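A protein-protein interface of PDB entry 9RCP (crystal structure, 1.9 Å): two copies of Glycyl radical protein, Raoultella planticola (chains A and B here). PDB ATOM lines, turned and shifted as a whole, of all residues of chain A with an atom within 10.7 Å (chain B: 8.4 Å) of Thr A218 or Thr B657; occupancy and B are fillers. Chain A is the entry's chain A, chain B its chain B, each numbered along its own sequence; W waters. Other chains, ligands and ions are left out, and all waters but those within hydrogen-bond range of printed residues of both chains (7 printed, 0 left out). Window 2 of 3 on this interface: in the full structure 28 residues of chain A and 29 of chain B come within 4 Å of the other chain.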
ATOM      1  N   LEU A 214       4.852 -27.364  -5.326  1.00  0.00           N
ATOM      2  CA  LEU A 214       4.269 -26.374  -4.424  1.00  0.00           C
ATOM      3  C   LEU A 214       5.300 -25.868  -3.423  1.00  0.00           C
ATOM      4  O   LEU A 214       5.981 -26.660  -2.763  1.00  0.00           O
ATOM      5  CB  LEU A 214       3.103 -26.969  -3.632  1.00  0.00           C
ATOM      6  CG  LEU A 214       1.661 -26.543  -3.849  1.00  0.00           C
ATOM      7  CD1 LEU A 214       0.794 -27.185  -2.757  1.00  0.00           C
ATOM      8  CD2 LEU A 214       1.569 -25.032  -3.824  1.00  0.00           C
ATOM      9  N   ASP A 215       5.369 -24.550  -3.263  1.00  0.00           N
ATOM     10  CA  ASP A 215       6.178 -23.982  -2.196  1.00  0.00           C
ATOM     11  C   ASP A 215       5.375 -24.121  -0.914  1.00  0.00           C
ATOM     12  O   ASP A 215       4.325 -23.487  -0.758  1.00  0.00           O
ATOM     13  CB  ASP A 215       6.540 -22.530  -2.478  1.00  0.00           C
ATOM     14  CG  ASP A 215       7.337 -21.892  -1.331  1.00  0.00           C
ATOM     15  OD1 ASP A 215       7.513 -22.536  -0.274  1.00  0.00           O
ATOM     16  OD2 ASP A 215       7.780 -20.737  -1.481  1.00  0.00           O
ATOM     17  N   ARG A 216       5.850 -24.966  -0.002  1.00  0.00           N
ATOM     18  CA  ARG A 216       5.122 -25.251   1.222  1.00  0.00           C
ATOM     19  C   ARG A 216       5.728 -24.565   2.434  1.00  0.00           C
ATOM     20  O   ARG A 216       5.475 -24.996   3.568  1.00  0.00           O
ATOM     21  CB  ARG A 216       5.051 -26.762   1.433  1.00  0.00           C
ATOM     22  CG  ARG A 216       4.291 -27.460   0.301  1.00  0.00           C
ATOM     23  CD  ARG A 216       4.409 -28.964   0.383  1.00  0.00           C
ATOM     24  NE  ARG A 216       3.853 -29.612  -0.807  1.00  0.00           N
ATOM     25  CZ  ARG A 216       2.612 -30.076  -0.851  1.00  0.00           C
ATOM     26  NH1 ARG A 216       1.842 -29.944   0.215  1.00  0.00           N
ATOM     27  NH2 ARG A 216       2.141 -30.666  -1.937  1.00  0.00           N
ATOM     28  N   SER A 217       6.504 -23.497   2.220  1.00  0.00           N
ATOM     29  CA  SER A 217       7.214 -22.831   3.308  1.00  0.00           C
ATOM     30  C   SER A 217       6.360 -21.825   4.074  1.00  0.00           C
ATOM     31  O   SER A 217       6.827 -21.295   5.094  1.00  0.00           O
ATOM     32  CB  SER A 217       8.475 -22.126   2.774  1.00  0.00           C
ATOM     33  OG  SER A 217       8.144 -21.069   1.875  1.00  0.00           O
ATOM     34  N   THR A 218       5.147 -21.524   3.611  1.00  0.00           N
ATOM     35  CA  THR A 218       4.292 -20.562   4.302  1.00  0.00           C
ATOM     36  C   THR A 218       2.910 -21.177   4.485  1.00  0.00           C
ATOM     37  O   THR A 218       2.752 -22.387   4.301  1.00  0.00           O
ATOM     38  CB  THR A 218       4.199 -19.232   3.537  1.00  0.00           C
ATOM     39  OG1 THR A 218       3.415 -19.397   2.355  1.00  0.00           O
ATOM     40  CG2 THR A 218       5.588 -18.719   3.136  1.00  0.00           C
ATOM     41  N   SER A 219       1.910 -20.382   4.876  1.00  0.00           N
ATOM     42  CA  SER A 219       0.557 -20.921   5.005  1.00  0.00           C
ATOM     43  C   SER A 219      -0.211 -20.967   3.684  1.00  0.00           C
ATOM     44  O   SER A 219      -1.257 -21.629   3.620  1.00  0.00           O
ATOM     45  CB  SER A 219      -0.264 -20.116   6.035  1.00  0.00           C
ATOM     46  OG  SER A 219      -0.425 -18.752   5.661  1.00  0.00           O
ATOM     47  N   ASP A 220       0.258 -20.300   2.626  1.00  0.00           N
ATOM     48  CA  ASP A 220      -0.493 -20.180   1.377  1.00  0.00           C
ATOM     49  C   ASP A 220      -0.708 -21.517   0.673  1.00  0.00           C
ATOM     50  O   ASP A 220      -1.635 -21.654  -0.135  1.00  0.00           O
ATOM     51  CB  ASP A 220       0.235 -19.226   0.427  1.00  0.00           C
ATOM     52  CG  ASP A 220       0.083 -17.773   0.834  1.00  0.00           C
ATOM     53  OD1 ASP A 220      -0.746 -17.481   1.720  1.00  0.00           O
ATOM     54  OD2 ASP A 220       0.803 -16.926   0.266  1.00  0.00           O
ATOM     55  N   TYR A 221       0.155 -22.502   0.918  1.00  0.00           N
ATOM     56  CA  TYR A 221       0.020 -23.769   0.201  1.00  0.00           C
ATOM     57  C   TYR A 221      -1.235 -24.541   0.584  1.00  0.00           C
ATOM     58  O   TYR A 221      -1.699 -25.364  -0.213  1.00  0.00           O
ATOM     59  CB  TYR A 221       1.282 -24.610   0.425  1.00  0.00           C
ATOM     60  CG  TYR A 221       1.333 -25.455   1.687  1.00  0.00           C
ATOM     61  CD1 TYR A 221       0.757 -26.726   1.754  1.00  0.00           C
ATOM     62  CD2 TYR A 221       2.010 -24.969   2.834  1.00  0.00           C
ATOM     63  CE1 TYR A 221       0.829 -27.478   2.909  1.00  0.00           C
ATOM     64  CE2 TYR A 221       2.096 -25.715   3.976  1.00  0.00           C
ATOM     65  CZ  TYR A 221       1.507 -26.961   4.025  1.00  0.00           C
ATOM     66  OH  TYR A 221       1.587 -27.690   5.201  1.00  0.00           O
ATOM     67  N   ILE A 222      -1.794 -24.289   1.769  1.00  0.00           N
ATOM     68  CA  ILE A 222      -2.867 -25.148   2.269  1.00  0.00           C
ATOM     69  C   ILE A 222      -4.092 -25.067   1.367  1.00  0.00           C
ATOM     70  O   ILE A 222      -4.636 -26.097   0.932  1.00  0.00           O
ATOM     71  CB  ILE A 222      -3.200 -24.794   3.725  1.00  0.00           C
ATOM     72  CG1 ILE A 222      -2.044 -25.220   4.636  1.00  0.00           C
ATOM     73  CG2 ILE A 222      -4.498 -25.465   4.169  1.00  0.00           C
ATOM     74  CD1 ILE A 222      -2.127 -24.632   6.050  1.00  0.00           C
ATOM     75  N   LYS A 223      -4.534 -23.842   1.052  1.00  0.00           N
ATOM     76  CA  LYS A 223      -5.696 -23.688   0.185  1.00  0.00           C
ATOM     77  C   LYS A 223      -5.375 -24.056  -1.261  1.00  0.00           C
ATOM     78  O   LYS A 223      -6.258 -24.533  -1.982  1.00  0.00           O
ATOM     79  CB  LYS A 223      -6.257 -22.261   0.278  1.00  0.00           C
ATOM     80  CG  LYS A 223      -7.038 -22.020   1.579  1.00  0.00           C
ATOM     81  CD  LYS A 223      -7.551 -20.589   1.709  1.00  0.00           C
ATOM     82  CE  LYS A 223      -8.770 -20.357   0.837  1.00  0.00           C
ATOM     83  NZ  LYS A 223      -9.958 -21.131   1.349  1.00  0.00           N
ATOM     84  N   LYS A 224      -4.130 -23.850  -1.702  1.00  0.00           N
ATOM     85  CA  LYS A 224      -3.771 -24.223  -3.068  1.00  0.00           C
ATOM     86  C   LYS A 224      -3.810 -25.733  -3.241  1.00  0.00           C
ATOM     87  O   LYS A 224      -4.218 -26.243  -4.292  1.00  0.00           O
ATOM     88  CB  LYS A 224      -2.390 -23.669  -3.415  1.00  0.00           C
ATOM     89  CG  LYS A 224      -2.368 -22.158  -3.523  1.00  0.00           C
ATOM     90  CD  LYS A 224      -0.949 -21.641  -3.549  1.00  0.00           C
ATOM     91  CE  LYS A 224      -0.265 -21.986  -4.851  1.00  0.00           C
ATOM     92  NZ  LYS A 224       1.099 -21.384  -4.930  1.00  0.00           N
ATOM     93  N   GLU A 225      -3.405 -26.463  -2.206  1.00  0.00           N
ATOM     94  CA  GLU A 225      -3.453 -27.912  -2.264  1.00  0.00           C
ATOM     95  C   GLU A 225      -4.899 -28.417  -2.225  1.00  0.00           C
ATOM     96  O   GLU A 225      -5.245 -29.380  -2.931  1.00  0.00           O
ATOM     97  CB  GLU A 225      -2.577 -28.455  -1.133  1.00  0.00           C
ATOM     98  CG  GLU A 225      -2.845 -29.804  -0.586  1.00  0.00           C
ATOM     99  CD  GLU A 225      -1.617 -30.323   0.163  1.00  0.00           C
ATOM    100  OE1 GLU A 225      -0.503 -30.314  -0.404  1.00  0.00           O
ATOM    101  OE2 GLU A 225      -1.747 -30.615   1.366  1.00  0.00           O
ATOM    102  N   HIS B 523       6.853 -29.008  10.594  1.00  0.00           N
ATOM    103  CA  HIS B 523       6.094 -28.609   9.410  1.00  0.00           C
ATOM    104  C   HIS B 523       4.649 -29.077   9.510  1.00  0.00           C
ATOM    105  O   HIS B 523       3.725 -28.333   9.160  1.00  0.00           O
ATOM    106  CB  HIS B 523       6.755 -29.158   8.137  1.00  0.00           C
ATOM    107  CG  HIS B 523       6.162 -28.612   6.868  1.00  0.00           C
ATOM    108  ND1 HIS B 523       5.102 -29.213   6.219  1.00  0.00           N
ATOM    109  CD2 HIS B 523       6.479 -27.521   6.132  1.00  0.00           C
ATOM    110  CE1 HIS B 523       4.790 -28.511   5.143  1.00  0.00           C
ATOM    111  NE2 HIS B 523       5.611 -27.481   5.065  1.00  0.00           N
ATOM    112  N   VAL B 526       2.752 -27.027  12.120  1.00  0.00           N
ATOM    113  CA  VAL B 526       2.381 -25.734  11.554  1.00  0.00           C
ATOM    114  C   VAL B 526       1.200 -25.876  10.595  1.00  0.00           C
ATOM    115  O   VAL B 526       0.285 -25.044  10.594  1.00  0.00           O
ATOM    116  CB  VAL B 526       3.612 -25.107  10.872  1.00  0.00           C
ATOM    117  CG1 VAL B 526       3.220 -23.891  10.005  1.00  0.00           C
ATOM    118  CG2 VAL B 526       4.642 -24.724  11.935  1.00  0.00           C
ATOM    119  N   GLU B 527       1.191 -26.932   9.776  1.00  0.00           N
ATOM    120  CA  GLU B 527       0.023 -27.224   8.938  1.00  0.00           C
ATOM    121  C   GLU B 527      -1.242 -27.363   9.765  1.00  0.00           C
ATOM    122  O   GLU B 527      -2.294 -26.806   9.417  1.00  0.00           O
ATOM    123  CB  GLU B 527       0.233 -28.518   8.154  1.00  0.00           C
ATOM    124  CG  GLU B 527      -0.646 -28.652   6.936  1.00  0.00           C
ATOM    125  CD  GLU B 527      -0.481 -29.999   6.242  1.00  0.00           C
ATOM    126  OE1 GLU B 527      -0.936 -31.063   6.753  1.00  0.00           O
ATOM    127  OE2 GLU B 527       0.244 -29.977   5.237  1.00  0.00           O
ATOM    128  N   CYS B 529      -1.882 -26.320  12.898  1.00  0.00           N
ATOM    129  CA  CYS B 529      -2.250 -25.016  13.463  1.00  0.00           C
ATOM    130  C   CYS B 529      -2.894 -24.125  12.413  1.00  0.00           C
ATOM    131  O   CYS B 529      -3.959 -23.546  12.648  1.00  0.00           O
ATOM    132  CB  CYS B 529      -1.015 -24.323  14.058  1.00  0.00           C
ATOM    133  SG  CYS B 529      -0.494 -25.083  15.615  1.00  0.00           S
ATOM    134  N   ASN B 530      -2.240 -23.977  11.256  1.00  0.00           N
ATOM    135  CA  ASN B 530      -2.755 -23.061  10.247  1.00  0.00           C
ATOM    136  C   ASN B 530      -4.096 -23.525   9.686  1.00  0.00           C
ATOM    137  O   ASN B 530      -4.932 -22.686   9.308  1.00  0.00           O
ATOM    138  CB  ASN B 530      -1.727 -22.846   9.134  1.00  0.00           C
ATOM    139  CG  ASN B 530      -0.542 -21.977   9.587  1.00  0.00           C
ATOM    140  OD1 ASN B 530      -0.630 -21.266  10.594  1.00  0.00           O
ATOM    141  ND2 ASN B 530       0.530 -21.972   8.806  1.00  0.00           N
ATOM    142  N   ASP B 533      -6.470 -22.269  12.058  1.00  0.00           N
ATOM    143  CA  ASP B 533      -6.494 -20.820  11.859  1.00  0.00           C
ATOM    144  C   ASP B 533      -7.417 -20.435  10.705  1.00  0.00           C
ATOM    145  O   ASP B 533      -8.298 -19.574  10.850  1.00  0.00           O
ATOM    146  CB  ASP B 533      -5.052 -20.346  11.606  1.00  0.00           C
ATOM    147  CG  ASP B 533      -4.786 -18.906  12.048  1.00  0.00           C
ATOM    148  OD1 ASP B 533      -5.710 -18.040  12.035  1.00  0.00           O
ATOM    149  OD2 ASP B 533      -3.623 -18.666  12.441  1.00  0.00           O
ATOM    150  N   ASN B 567       0.619 -10.467  15.279  1.00  0.00           N
ATOM    151  CA  ASN B 567       0.037 -11.781  15.043  1.00  0.00           C
ATOM    152  C   ASN B 567       1.086 -12.862  15.262  1.00  0.00           C
ATOM    153  O   ASN B 567       2.182 -12.799  14.691  1.00  0.00           O
ATOM    154  CB  ASN B 567      -0.542 -11.868  13.626  1.00  0.00           C
ATOM    155  CG  ASN B 567      -1.875 -11.138  13.511  1.00  0.00           C
ATOM    156  OD1 ASN B 567      -2.915 -11.645  13.932  1.00  0.00           O
ATOM    157  ND2 ASN B 567      -1.834  -9.914  12.994  1.00  0.00           N
ATOM    158  N   PHE B 568       0.738 -13.858  16.068  1.00  0.00           N
ATOM    159  CA  PHE B 568       1.630 -14.971  16.372  1.00  0.00           C
ATOM    160  C   PHE B 568       0.819 -16.255  16.453  1.00  0.00           C
ATOM    161  O   PHE B 568      -0.413 -16.238  16.498  1.00  0.00           O
ATOM    162  CB  PHE B 568       2.393 -14.744  17.700  1.00  0.00           C
ATOM    163  CG  PHE B 568       3.141 -13.439  17.752  1.00  0.00           C
ATOM    164  CD1 PHE B 568       4.232 -13.222  16.937  1.00  0.00           C
ATOM    165  CD2 PHE B 568       2.718 -12.409  18.590  1.00  0.00           C
ATOM    166  CE1 PHE B 568       4.914 -12.013  16.959  1.00  0.00           C
ATOM    167  CE2 PHE B 568       3.397 -11.193  18.628  1.00  0.00           C
ATOM    168  CZ  PHE B 568       4.498 -10.994  17.810  1.00  0.00           C
ATOM    169  N   THR B 569       1.536 -17.378  16.452  1.00  0.00           N
ATOM    170  CA  THR B 569       0.994 -18.681  16.796  1.00  0.00           C
ATOM    171  C   THR B 569       1.978 -19.351  17.746  1.00  0.00           C
ATOM    172  O   THR B 569       3.172 -19.400  17.435  1.00  0.00           O
ATOM    173  CB  THR B 569       0.814 -19.566  15.558  1.00  0.00           C
ATOM    174  OG1 THR B 569      -0.035 -18.896  14.622  1.00  0.00           O
ATOM    175  CG2 THR B 569       0.201 -20.911  15.991  1.00  0.00           C
ATOM    176  N   GLU B 652      13.317 -24.331  14.945  1.00  0.00           N
ATOM    177  CA  GLU B 652      12.474 -24.816  13.847  1.00  0.00           C
ATOM    178  C   GLU B 652      11.143 -24.079  13.810  1.00  0.00           C
ATOM    179  O   GLU B 652      10.704 -23.632  12.747  1.00  0.00           O
ATOM    180  CB  GLU B 652      12.204 -26.317  13.958  1.00  0.00           C
ATOM    181  CG  GLU B 652      13.158 -27.158  13.188  1.00  0.00           C
ATOM    182  CD  GLU B 652      13.191 -26.829  11.711  1.00  0.00           C
ATOM    183  OE1 GLU B 652      12.157 -26.894  11.013  1.00  0.00           O
ATOM    184  OE2 GLU B 652      14.274 -26.419  11.269  1.00  0.00           O
ATOM    185  N   VAL B 653      10.471 -23.994  14.966  1.00  0.00           N
ATOM    186  CA  VAL B 653       9.158 -23.350  15.061  1.00  0.00           C
ATOM    187  C   VAL B 653       9.182 -21.950  14.462  1.00  0.00           C
ATOM    188  O   VAL B 653       8.294 -21.578  13.686  1.00  0.00           O
ATOM    189  CB  VAL B 653       8.684 -23.319  16.526  1.00  0.00           C
ATOM    190  CG1 VAL B 653       7.381 -22.473  16.678  1.00  0.00           C
ATOM    191  CG2 VAL B 653       8.447 -24.734  17.011  1.00  0.00           C
ATOM    192  N   GLU B 654      10.197 -21.147  14.811  1.00  0.00           N
ATOM    193  CA  GLU B 654      10.146 -19.736  14.412  1.00  0.00           C
ATOM    194  C   GLU B 654      10.393 -19.524  12.921  1.00  0.00           C
ATOM    195  O   GLU B 654      10.311 -18.381  12.455  1.00  0.00           O
ATOM    196  CB  GLU B 654      11.149 -18.904  15.232  1.00  0.00           C
ATOM    197  CG  GLU B 654      12.590 -19.451  15.186  1.00  0.00           C
ATOM    198  CD  GLU B 654      13.671 -18.442  15.592  1.00  0.00           C
ATOM    199  OE1 GLU B 654      14.823 -18.595  15.122  1.00  0.00           O
ATOM    200  OE2 GLU B 654      13.384 -17.518  16.384  1.00  0.00           O
ATOM    201  N   LYS B 655      10.669 -20.579  12.157  1.00  0.00           N
ATOM    202  CA  LYS B 655      10.828 -20.445  10.712  1.00  0.00           C
ATOM    203  C   LYS B 655       9.506 -20.250   9.976  1.00  0.00           C
ATOM    204  O   LYS B 655       9.528 -19.982   8.769  1.00  0.00           O
ATOM    205  CB  LYS B 655      11.545 -21.679  10.147  1.00  0.00           C
ATOM    206  CG  LYS B 655      12.966 -21.849  10.642  1.00  0.00           C
ATOM    207  CD  LYS B 655      13.556 -23.161  10.126  1.00  0.00           C
ATOM    208  CE  LYS B 655      14.963 -23.385  10.628  1.00  0.00           C
ATOM    209  NZ  LYS B 655      15.524 -24.696  10.171  1.00  0.00           N
ATOM    210  N   TYR B 656       8.369 -20.352  10.663  1.00  0.00           N
ATOM    211  CA  TYR B 656       7.069 -20.475  10.016  1.00  0.00           C
ATOM    212  C   TYR B 656       6.161 -19.287  10.325  1.00  0.00           C
ATOM    213  O   TYR B 656       6.396 -18.521  11.269  1.00  0.00           O
ATOM    214  CB  TYR B 656       6.398 -21.791  10.431  1.00  0.00           C
ATOM    215  CG  TYR B 656       7.163 -22.968   9.884  1.00  0.00           C
ATOM    216  CD1 TYR B 656       6.998 -23.364   8.552  1.00  0.00           C
ATOM    217  CD2 TYR B 656       8.098 -23.650  10.665  1.00  0.00           C
ATOM    218  CE1 TYR B 656       7.711 -24.423   8.024  1.00  0.00           C
ATOM    219  CE2 TYR B 656       8.842 -24.727  10.119  1.00  0.00           C
ATOM    220  CZ  TYR B 656       8.624 -25.107   8.807  1.00  0.00           C
ATOM    221  OH  TYR B 656       9.330 -26.166   8.248  1.00  0.00           O
ATOM    222  N   THR B 657       5.128 -19.134   9.482  1.00  0.00           N
ATOM    223  CA  THR B 657       4.158 -18.047   9.559  1.00  0.00           C
ATOM    224  C   THR B 657       2.735 -18.591   9.486  1.00  0.00           C
ATOM    225  O   THR B 657       2.499 -19.711   9.023  1.00  0.00           O
ATOM    226  CB  THR B 657       4.350 -17.018   8.418  1.00  0.00           C
ATOM    227  OG1 THR B 657       4.314 -17.684   7.152  1.00  0.00           O
ATOM    228  CG2 THR B 657       5.675 -16.247   8.561  1.00  0.00           C
ATOM    229  N   ASN B 658       1.777 -17.772   9.907  1.00  0.00           N
ATOM    230  CA  ASN B 658       0.370 -18.136   9.904  1.00  0.00           C
ATOM    231  C   ASN B 658      -0.419 -17.292   8.892  1.00  0.00           C
ATOM    232  O   ASN B 658       0.131 -16.377   8.269  1.00  0.00           O
ATOM    233  CB  ASN B 658      -0.197 -18.027  11.333  1.00  0.00           C
ATOM    234  CG  ASN B 658      -0.131 -16.626  11.900  1.00  0.00           C
ATOM    235  OD1 ASN B 658      -0.381 -15.625  11.216  1.00  0.00           O
ATOM    236  ND2 ASN B 658       0.255 -16.549  13.180  1.00  0.00           N
ATOM    237  N   PRO B 659      -1.694 -17.628   8.643  1.00  0.00           N
ATOM    238  CA  PRO B 659      -2.444 -16.906   7.598  1.00  0.00           C
ATOM    239  C   PRO B 659      -2.823 -15.483   7.981  1.00  0.00           C
ATOM    240  O   PRO B 659      -3.339 -14.749   7.125  1.00  0.00           O
ATOM    241  CB  PRO B 659      -3.708 -17.764   7.401  1.00  0.00           C
ATOM    242  CG  PRO B 659      -3.375 -19.097   8.012  1.00  0.00           C
ATOM    243  CD  PRO B 659      -2.478 -18.768   9.159  1.00  0.00           C
ATOM    244  N   ARG B 660      -2.585 -15.070   9.218  1.00  0.00           N
ATOM    245  CA  ARG B 660      -2.825 -13.701   9.636  1.00  0.00           C
ATOM    246  C   ARG B 660      -1.614 -12.810   9.402  1.00  0.00           C
ATOM    247  O   ARG B 660      -1.600 -11.681   9.885  1.00  0.00           O
ATOM    248  CB  ARG B 660      -3.229 -13.665  11.120  1.00  0.00           C
ATOM    249  CG  ARG B 660      -4.605 -14.293  11.370  1.00  0.00           C
ATOM    250  CD  ARG B 660      -4.814 -14.615  12.828  1.00  0.00           C
ATOM    251  NE  ARG B 660      -4.102 -15.818  13.267  1.00  0.00           N
ATOM    252  CZ  ARG B 660      -3.114 -15.811  14.161  1.00  0.00           C
ATOM    253  NH1 ARG B 660      -2.706 -14.663  14.716  1.00  0.00           N
ATOM    254  NH2 ARG B 660      -2.547 -16.946  14.530  1.00  0.00           N
ATOM    255  N   GLY B 661      -0.601 -13.291   8.681  1.00  0.00           N
ATOM    256  CA  GLY B 661       0.594 -12.504   8.446  1.00  0.00           C
ATOM    257  C   GLY B 661       1.549 -12.446   9.621  1.00  0.00           C
ATOM    258  O   GLY B 661       2.372 -11.526   9.701  1.00  0.00           O
ATOM    259  N   GLY B 662       1.446 -13.394  10.550  1.00  0.00           N
ATOM    260  CA  GLY B 662       2.246 -13.407  11.750  1.00  0.00           C
ATOM    261  C   GLY B 662       3.171 -14.613  11.825  1.00  0.00           C
ATOM    262  O   GLY B 662       3.266 -15.423  10.904  1.00  0.00           O
ATOM    263  N   ARG B 663       3.845 -14.720  12.957  1.00  0.00           N
ATOM    264  CA  ARG B 663       5.001 -15.590  13.101  1.00  0.00           C
ATOM    265  C   ARG B 663       4.764 -16.617  14.202  1.00  0.00           C
ATOM    266  O   ARG B 663       4.268 -16.274  15.283  1.00  0.00           O
ATOM    267  CB  ARG B 663       6.231 -14.722  13.406  1.00  0.00           C
ATOM    268  CG  ARG B 663       7.500 -15.450  13.807  1.00  0.00           C
ATOM    269  CD  ARG B 663       8.146 -16.112  12.622  1.00  0.00           C
ATOM    270  NE  ARG B 663       8.372 -15.177  11.519  1.00  0.00           N
ATOM    271  CZ  ARG B 663       8.914 -15.525  10.356  1.00  0.00           C
ATOM    272  NH1 ARG B 663       9.289 -16.776  10.148  1.00  0.00           N
ATOM    273  NH2 ARG B 663       9.086 -14.624   9.400  1.00  0.00           N
ATOM    274  N   PHE B 664       5.157 -17.876  13.948  1.00  0.00           N
ATOM    275  CA  PHE B 664       5.204 -18.869  15.009  1.00  0.00           C
ATOM    276  C   PHE B 664       6.359 -18.589  15.961  1.00  0.00           C
ATOM    277  O   PHE B 664       7.435 -18.144  15.562  1.00  0.00           O
ATOM    278  CB  PHE B 664       5.363 -20.302  14.482  1.00  0.00           C
ATOM    279  CG  PHE B 664       4.119 -20.888  13.882  1.00  0.00           C
ATOM    280  CD1 PHE B 664       3.526 -20.330  12.747  1.00  0.00           C
ATOM    281  CD2 PHE B 664       3.489 -21.954  14.507  1.00  0.00           C
ATOM    282  CE1 PHE B 664       2.356 -20.881  12.220  1.00  0.00           C
ATOM    283  CE2 PHE B 664       2.336 -22.505  13.986  1.00  0.00           C
ATOM    284  CZ  PHE B 664       1.764 -21.973  12.841  1.00  0.00           C
ATOM    285  N   GLN B 665       6.129 -18.887  17.234  1.00  0.00           N
ATOM    286  CA  GLN B 665       7.148 -18.715  18.261  1.00  0.00           C
ATOM    287  C   GLN B 665       6.885 -19.780  19.305  1.00  0.00           C
ATOM    288  O   GLN B 665       5.740 -19.968  19.729  1.00  0.00           O
ATOM    289  CB  GLN B 665       7.089 -17.297  18.866  1.00  0.00           C
ATOM    290  CG  GLN B 665       5.677 -16.896  19.259  1.00  0.00           C
ATOM    291  CD  GLN B 665       5.582 -15.603  20.082  1.00  0.00           C
ATOM    292  OE1 GLN B 665       6.566 -14.894  20.294  1.00  0.00           O
ATOM    293  NE2 GLN B 665       4.401 -15.347  20.602  1.00  0.00           N
HETATM  294  O   HOH W   1       0.439 -31.169   3.038  1.00  0.00           O
HETATM  295  O   HOH W   2       9.529 -21.394   6.252  1.00  0.00           O
HETATM  296  O   HOH W   3       4.312 -21.343   7.404  1.00  0.00           O
HETATM  297  O   HOH W   4       1.988 -17.493   5.655  1.00  0.00           O
HETATM  298  O   HOH W   5       6.700 -19.037   6.807  1.00  0.00           O
HETATM  299  O   HOH W   6       1.486 -23.849   6.833  1.00  0.00           O
HETATM  300  O   HOH W   7       3.195 -26.293   7.195  1.00  0.00           O
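A ring nitrogen (NE2) of His B523 lies within hydrogen-bond range of the backbone carbonyl oxygen (O) of Arg A216, 2.9 Å away.
The side-chain hydroxyl (OH) of Tyr A221 sits at hydrogen-bond distance from the side-chain carboxylate (OE2) of Glu B527 (2.7 Å).
The backbone nitrogen of Pro B659 lies close to the side-chain hydroxyl of Ser A219, 3.4 Å away.
The guanidinium group (NH1) of Arg A216 is in salt-bridge range of the side-chain carboxylate (OE1) of Glu A225 (2.5 Å).
OG1 of Thr A218 sits at hydrogen-bond distance from N of Asp A220 (3.3 Å).
ND2 of Asn B530 lies within hydrogen-bond range of O of Thr B657, 3.0 Å away.
OD1 of Asn B658 sits at hydrogen-bond distance from N of Arg B660, 3.0 Å away.
OD1 of Asn B658 lies within hydrogen-bond range of N of Gly B661.
N of Gly B662 lies within hydrogen-bond range of OD1 of Asn B658.
Among the printed residues, pairs that only touch across the chains: Tyr A221 with His B523, Ser A219 with Asn B530, Ser A219 with Asn B658, Ile A222 with Asn B530 and Thr A218 with Thr B657.
Of chain B, only Thr B657 comes within 4 Å of Thr A218.
Thr B657 touches one residue of chain A.
Ser A217 touches none of the printed residues of chain B.
Asn B658 touches just one residue of chain A: Ser A219 (3.5 Å).
No residue of chain A comes within 4 Å of Gly B661.
No residue of chain A comes within 4 Å of Arg B663.
No residue of chain A comes within 4 Å of Phe B664.
Printed residues of chain A within 4 Å of Glu B527: Tyr A221.
Of the printed residues of chain A, Asn B530 touches Ser A219 (3.4 Å) and Ile A222 (3.6 Å).
Glu B652 touches none of the printed residues of chain A.
The nearest residue of chain B that does not touch Thr A218 is Asn B530 (5.0 Å).
Hydrophobic or aromatic side chains of chain B within 4 Å of the printed part of chain A: His B523 and Pro B659.
Printed residues of chain A that touch a printed residue of chain B: Arg A216, Thr A218, Ser A219, Tyr A221 and Ile A222.
Hydrophobic or aromatic side chains of chain A that line the printed part of chain B: Tyr A221 and Ile A222.
Among the printed residues, no Asp or Glu carboxylate lies within 4 Å of a Lys or Arg side-chain nitrogen of the other chain.
No position is printed for both chains.
Water W1 lies within hydrogen-bond range of OE2 of Glu B527 (2.5 Å), OE2 of Glu A225 (2.8 Å) and NH1 of Arg A216 (3.4 Å).
Water W4 lies within hydrogen-bond range of the side-chain hydroxyl (OG) of Ser A219 (2.7 Å), the side-chain hydroxyl (OG1) of Thr B657 (2.8 Å) and the backbone carbonyl oxygen (O) of Asn B658 (3.4 Å).
Water W5 lies within hydrogen-bond range of OG1 of Thr B657 (2.8 Å) and O of Ser A217 (2.8 Å).
Water W7 lies within hydrogen-bond range of O of His B523 (2.9 Å), OH of Tyr A221 (2.9 Å) and N of Glu B527 (3.3 Å).
Water W2 lies within hydrogen-bond range of the backbone carbonyl oxygen of Lys B655 (2.9 Å) and the backbone carbonyl oxygen of Ser A217 (2.9 Å).
Water W6 lies within hydrogen-bond range of the side-chain amide nitrogen of Asn B530 (2.9 Å) and the backbone carbonyl oxygen of Thr A218 (3.2 Å).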
